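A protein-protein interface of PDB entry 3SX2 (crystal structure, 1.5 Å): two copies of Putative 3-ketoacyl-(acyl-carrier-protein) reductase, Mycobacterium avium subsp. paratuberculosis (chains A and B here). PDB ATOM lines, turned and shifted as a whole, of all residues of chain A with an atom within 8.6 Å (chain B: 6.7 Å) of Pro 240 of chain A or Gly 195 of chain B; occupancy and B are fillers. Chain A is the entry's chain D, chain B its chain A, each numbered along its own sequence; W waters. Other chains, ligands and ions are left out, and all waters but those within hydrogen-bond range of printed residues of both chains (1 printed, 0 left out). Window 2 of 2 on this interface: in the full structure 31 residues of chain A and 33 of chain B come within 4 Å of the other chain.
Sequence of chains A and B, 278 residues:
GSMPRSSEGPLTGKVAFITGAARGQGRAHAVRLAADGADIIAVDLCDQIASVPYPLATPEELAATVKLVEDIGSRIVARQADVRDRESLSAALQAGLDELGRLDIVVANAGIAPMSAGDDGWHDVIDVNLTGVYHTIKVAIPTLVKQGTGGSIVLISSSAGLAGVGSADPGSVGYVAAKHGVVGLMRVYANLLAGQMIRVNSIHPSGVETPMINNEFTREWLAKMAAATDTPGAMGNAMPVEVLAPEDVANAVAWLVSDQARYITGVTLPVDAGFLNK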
ATOM      1  N   GLY A 236      11.481  -3.867 -19.578  1.00  0.00           N
ATOM      2  CA  GLY A 236      10.950  -3.916 -18.216  1.00  0.00           C
ATOM      3  C   GLY A 236      12.040  -3.943 -17.153  1.00  0.00           C
ATOM      4  O   GLY A 236      13.185  -4.204 -17.399  1.00  0.00           O
ATOM      5  N   ASN A 237      11.610  -3.685 -15.934  1.00  0.00           N
ATOM      6  CA  ASN A 237      12.487  -3.815 -14.775  1.00  0.00           C
ATOM      7  C   ASN A 237      12.705  -5.294 -14.449  1.00  0.00           C
ATOM      8  O   ASN A 237      11.994  -6.184 -14.949  1.00  0.00           O
ATOM      9  CB  ASN A 237      11.865  -3.075 -13.594  1.00  0.00           C
ATOM     10  CG  ASN A 237      11.730  -1.594 -13.845  1.00  0.00           C
ATOM     11  OD1 ASN A 237      12.621  -0.983 -14.425  1.00  0.00           O
ATOM     12  ND2 ASN A 237      10.625  -0.997 -13.391  1.00  0.00           N
ATOM     13  N   ALA A 238      13.707  -5.589 -13.611  1.00  0.00           N
ATOM     14  CA  ALA A 238      13.922  -6.968 -13.179  1.00  0.00           C
ATOM     15  C   ALA A 238      12.879  -7.432 -12.145  1.00  0.00           C
ATOM     16  O   ALA A 238      12.312  -8.509 -12.276  1.00  0.00           O
ATOM     17  CB  ALA A 238      15.367  -7.146 -12.645  1.00  0.00           C
ATOM     18  N   MET A 239      12.634  -6.615 -11.131  1.00  0.00           N
ATOM     19  CA  MET A 239      11.567  -6.850 -10.187  1.00  0.00           C
ATOM     20  C   MET A 239      10.239  -6.570 -10.881  1.00  0.00           C
ATOM     21  O   MET A 239      10.164  -5.716 -11.764  1.00  0.00           O
ATOM     22  CB  MET A 239      11.697  -5.932  -8.978  1.00  0.00           C
ATOM     23  CG  MET A 239      12.977  -6.104  -8.207  1.00  0.00           C
ATOM     24  SD  MET A 239      13.308  -4.859  -6.917  1.00  0.00           S
ATOM     25  CE  MET A 239      12.199  -5.408  -5.613  1.00  0.00           C
ATOM     26  N   PRO A 240       9.182  -7.294 -10.489  1.00  0.00           N
ATOM     27  CA  PRO A 240       7.870  -7.122 -11.131  1.00  0.00           C
ATOM     28  C   PRO A 240       7.143  -5.839 -10.672  1.00  0.00           C
ATOM     29  O   PRO A 240       6.089  -5.871  -9.997  1.00  0.00           O
ATOM     30  CB  PRO A 240       7.144  -8.410 -10.714  1.00  0.00           C
ATOM     31  CG  PRO A 240       7.698  -8.748  -9.429  1.00  0.00           C
ATOM     32  CD  PRO A 240       9.191  -8.445  -9.573  1.00  0.00           C
ATOM     33  N   VAL A 241       7.756  -4.711 -11.048  1.00  0.00           N
ATOM     34  CA  VAL A 241       7.335  -3.347 -10.743  1.00  0.00           C
ATOM     35  C   VAL A 241       7.184  -2.641 -12.087  1.00  0.00           C
ATOM     36  O   VAL A 241       8.143  -2.521 -12.855  1.00  0.00           O
ATOM     37  CB  VAL A 241       8.430  -2.636  -9.875  1.00  0.00           C
ATOM     38  CG1 VAL A 241       8.090  -1.164  -9.718  1.00  0.00           C
ATOM     39  CG2 VAL A 241       8.623  -3.357  -8.532  1.00  0.00           C
ATOM     40  N   GLU A 242       5.950  -2.245 -12.427  1.00  0.00           N
ATOM     41  CA  GLU A 242       5.664  -1.629 -13.734  1.00  0.00           C
ATOM     42  C   GLU A 242       6.382  -0.303 -13.881  1.00  0.00           C
ATOM     43  O   GLU A 242       6.953  -0.017 -14.920  1.00  0.00           O
ATOM     44  CB  GLU A 242       4.142  -1.424 -13.940  1.00  0.00           C
ATOM     45  N   VAL A 243       6.340   0.501 -12.829  1.00  0.00           N
ATOM     46  CA  VAL A 243       6.855   1.857 -12.842  1.00  0.00           C
ATOM     47  C   VAL A 243       7.138   2.256 -11.393  1.00  0.00           C
ATOM     48  O   VAL A 243       6.450   1.795 -10.471  1.00  0.00           O
ATOM     49  CB  VAL A 243       5.786   2.809 -13.453  1.00  0.00           C
ATOM     50  CG1 VAL A 243       4.602   3.018 -12.518  1.00  0.00           C
ATOM     51  CG2 VAL A 243       6.425   4.157 -13.839  1.00  0.00           C
ATOM     52  N   ALA A 273      14.585  -0.765  -9.838  1.00  0.00           N
ATOM     53  CA  ALA A 273      13.989  -2.107  -9.744  1.00  0.00           C
ATOM     54  C   ALA A 273      14.782  -3.138 -10.545  1.00  0.00           C
ATOM     55  O   ALA A 273      14.248  -4.115 -11.056  1.00  0.00           O
ATOM     56  CB  ALA A 273      12.491  -2.078 -10.140  1.00  0.00           C
ATOM     57  N   GLY A 274      16.089  -2.913 -10.629  1.00  0.00           N
ATOM     58  CA  GLY A 274      17.018  -3.813 -11.286  1.00  0.00           C
ATOM     59  C   GLY A 274      17.210  -3.645 -12.781  1.00  0.00           C
ATOM     60  O   GLY A 274      17.877  -4.467 -13.400  1.00  0.00           O
ATOM     61  N   LYS A 278      19.701  -5.960 -15.395  1.00  0.00           N
ATOM     62  CA  LYS A 278      18.932  -7.056 -16.019  1.00  0.00           C
ATOM     63  C   LYS A 278      19.654  -7.523 -17.275  1.00  0.00           C
ATOM     64  O   LYS A 278      20.188  -6.685 -18.006  1.00  0.00           O
ATOM     65  CB  LYS A 278      17.472  -6.579 -16.311  1.00  0.00           C
ATOM     66  CG  LYS A 278      16.490  -7.680 -16.761  1.00  0.00           C
ATOM     67  CD  LYS A 278      15.133  -7.027 -17.131  1.00  0.00           C
ATOM     68  CE  LYS A 278      14.079  -8.018 -17.610  1.00  0.00           C
ATOM     69  NZ  LYS A 278      12.630  -7.581 -17.382  1.00  0.00           N
ATOM     70  OXT LYS A 278      19.727  -8.735 -17.572  1.00  0.00           O
ATOM     71  N   ALA B 190      20.820 -10.933  -7.977  1.00  0.00           N
ATOM     72  CA  ALA B 190      19.813  -9.879  -8.129  1.00  0.00           C
ATOM     73  C   ALA B 190      18.854 -10.270  -9.259  1.00  0.00           C
ATOM     74  O   ALA B 190      17.623 -10.116  -9.156  1.00  0.00           O
ATOM     75  CB  ALA B 190      20.472  -8.519  -8.389  1.00  0.00           C
ATOM     76  N   ASN B 191      19.401 -10.826 -10.348  1.00  0.00           N
ATOM     77  CA  ASN B 191      18.543 -11.266 -11.457  1.00  0.00           C
ATOM     78  C   ASN B 191      17.722 -12.499 -11.143  1.00  0.00           C
ATOM     79  O   ASN B 191      16.535 -12.548 -11.498  1.00  0.00           O
ATOM     80  CB  ASN B 191      19.375 -11.439 -12.737  1.00  0.00           C
ATOM     81  CG  ASN B 191      19.723 -10.105 -13.396  1.00  0.00           C
ATOM     82  OD1 ASN B 191      18.897  -9.185 -13.396  1.00  0.00           O
ATOM     83  ND2 ASN B 191      20.909 -10.003 -13.987  1.00  0.00           N
ATOM     84  N   LEU B 192      18.320 -13.483 -10.499  1.00  0.00           N
ATOM     85  CA  LEU B 192      17.624 -14.749 -10.163  1.00  0.00           C
ATOM     86  C   LEU B 192      16.496 -14.534  -9.165  1.00  0.00           C
ATOM     87  O   LEU B 192      15.479 -15.258  -9.228  1.00  0.00           O
ATOM     88  CB  LEU B 192      18.596 -15.769  -9.586  1.00  0.00           C
ATOM     89  CG  LEU B 192      19.638 -16.351 -10.566  1.00  0.00           C
ATOM     90  CD1 LEU B 192      20.704 -17.113  -9.833  1.00  0.00           C
ATOM     91  CD2 LEU B 192      18.948 -17.240 -11.595  1.00  0.00           C
ATOM     92  N   LEU B 193      16.657 -13.555  -8.271  1.00  0.00           N
ATOM     93  CA  LEU B 193      15.757 -13.378  -7.119  1.00  0.00           C
ATOM     94  C   LEU B 193      14.792 -12.187  -7.273  1.00  0.00           C
ATOM     95  O   LEU B 193      13.922 -12.032  -6.444  1.00  0.00           O
ATOM     96  CB  LEU B 193      16.535 -13.247  -5.809  1.00  0.00           C
ATOM     97  CG  LEU B 193      17.389 -14.463  -5.476  1.00  0.00           C
ATOM     98  CD1 LEU B 193      18.210 -14.194  -4.227  1.00  0.00           C
ATOM     99  CD2 LEU B 193      16.560 -15.747  -5.273  1.00  0.00           C
ATOM    100  N   ALA B 194      14.953 -11.361  -8.307  1.00  0.00           N
ATOM    101  CA  ALA B 194      14.127 -10.174  -8.511  1.00  0.00           C
ATOM    102  C   ALA B 194      12.653 -10.507  -8.551  1.00  0.00           C
ATOM    103  O   ALA B 194      11.819  -9.761  -8.031  1.00  0.00           O
ATOM    104  CB  ALA B 194      14.537  -9.471  -9.811  1.00  0.00           C
ATOM    105  N   GLY B 195      12.315 -11.611  -9.186  1.00  0.00           N
ATOM    106  CA  GLY B 195      10.888 -11.991  -9.316  1.00  0.00           C
ATOM    107  C   GLY B 195      10.235 -12.305  -7.987  1.00  0.00           C
ATOM    108  O   GLY B 195       9.003 -12.308  -7.889  1.00  0.00           O
ATOM    109  N   GLN B 196      11.040 -12.645  -6.992  1.00  0.00           N
ATOM    110  CA  GLN B 196      10.590 -12.895  -5.619  1.00  0.00           C
ATOM    111  C   GLN B 196      10.612 -11.631  -4.749  1.00  0.00           C
ATOM    112  O   GLN B 196      10.398 -11.724  -3.547  1.00  0.00           O
ATOM    113  CB  GLN B 196      11.468 -13.960  -4.935  1.00  0.00           C
ATOM    114  CG  GLN B 196      11.660 -15.251  -5.717  1.00  0.00           C
ATOM    115  CD  GLN B 196      10.356 -15.886  -6.152  1.00  0.00           C
ATOM    116  OE1 GLN B 196       9.433 -16.084  -5.345  1.00  0.00           O
ATOM    117  NE2 GLN B 196      10.247 -16.185  -7.457  1.00  0.00           N
ATOM    118  N   MET B 197      10.908 -10.485  -5.341  1.00  0.00           N
ATOM    119  CA  MET B 197      11.018  -9.213  -4.605  1.00  0.00           C
ATOM    120  C   MET B 197      12.099  -9.262  -3.539  1.00  0.00           C
ATOM    121  O   MET B 197      12.010  -8.588  -2.508  1.00  0.00           O
ATOM    122  CB  MET B 197       9.662  -8.752  -4.022  1.00  0.00           C
ATOM    123  CG  MET B 197       8.598  -8.549  -5.083  1.00  0.00           C
ATOM    124  SD  MET B 197       8.872  -7.157  -6.202  1.00  0.00           S
ATOM    125  CE  MET B 197       8.526  -5.769  -5.148  1.00  0.00           C
ATOM    126  N   ILE B 198      13.164 -10.025  -3.806  1.00  0.00           N
ATOM    127  CA  ILE B 198      14.329 -10.083  -2.937  1.00  0.00           C
ATOM    128  C   ILE B 198      15.408  -9.213  -3.584  1.00  0.00           C
ATOM    129  O   ILE B 198      15.860  -9.537  -4.695  1.00  0.00           O
ATOM    130  CB  ILE B 198      14.844 -11.526  -2.723  1.00  0.00           C
ATOM    131  CG1 ILE B 198      13.819 -12.390  -1.984  1.00  0.00           C
ATOM    132  CG2 ILE B 198      16.173 -11.537  -1.934  1.00  0.00           C
ATOM    133  CD1 ILE B 198      14.038 -13.902  -2.184  1.00  0.00           C
HETATM  134  O   HOH W   1      18.649  -6.813 -11.859  1.00  0.00           O
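Pro 240 of chain A touches just these residues of chain B: Ala 194, Gly 195 and Met 197.
Printed residues of chain A within 4 Å of Gly 195 of chain B: Pro 240.
Of the printed residues of chain B, Lys 278 of chain A touches Asn 191.
Of the printed residues of chain A, Met 197 of chain B touches Met 239 (3.7 Å) and Pro 240 (3.6 Å).
Val 241 of chain A touches none of the printed residues of chain B.
Ala 190 of chain B touches none of the printed residues of chain A.
The nearest residue of chain B that does not touch Pro 240 of chain A is Gln 196 of chain B (5.3 Å).
The nearest residue of chain A that does not touch Gly 195 of chain B is Ala 238 of chain A (4.4 Å).
The nearest printed residue of chain A that does not touch Met 197 of chain B is Val 241 of chain A (4.2 Å).
Hydrophobic or aromatic side chains of chain B that line the printed part of chain A: Ala 194 and Met 197.
Among the printed residues, no Asp or Glu carboxylate lies within 4 Å of a Lys or Arg side-chain nitrogen of the other chain.
Water W1 bridges the side-chain amide oxygen of Asn 191 of chain B and the backbone carbonyl oxygen of Gly 274 of chain A.
Among the printed residues, merely in contact across the chains: Ala 238 of chain A with Ala 194 of chain B, Met 239 of chain A with Ala 194 of chain B, Met 239 of chain A with Met 197 of chain B, Pro 240 of chain A with Ala 194 of chain B, Pro 240 of chain A with Gly 195 of chain B, Pro 240 of chain A with Met 197 of chain B and Lys 278 of chain A with Asn 191 of chain B.
No position is printed for both chains.
Of the 7 pairs that touch across the chains among the printed residues, none has its exchanged pair printed and touching as well.
The backbone carbonyl oxygen (O) of Asn 237 of chain A sits at hydrogen-bond distance from the side-chain amino group (NZ) of Lys 278 of chain A, at 2.9 Å.
N of Met 239 of chain A sits at hydrogen-bond distance from O of Ala 273 of chain A, 3.0 Å away.
The side-chain amino group (NZ) of Lys 278 of chain A lies within hydrogen-bond range of the backbone carbonyl oxygen (O) of Gly 236 of chain A (3.4 Å).
O of Ala 273 of chain A sits at hydrogen-bond distance from N of Ala 238 of chain A, 3.0 Å away.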
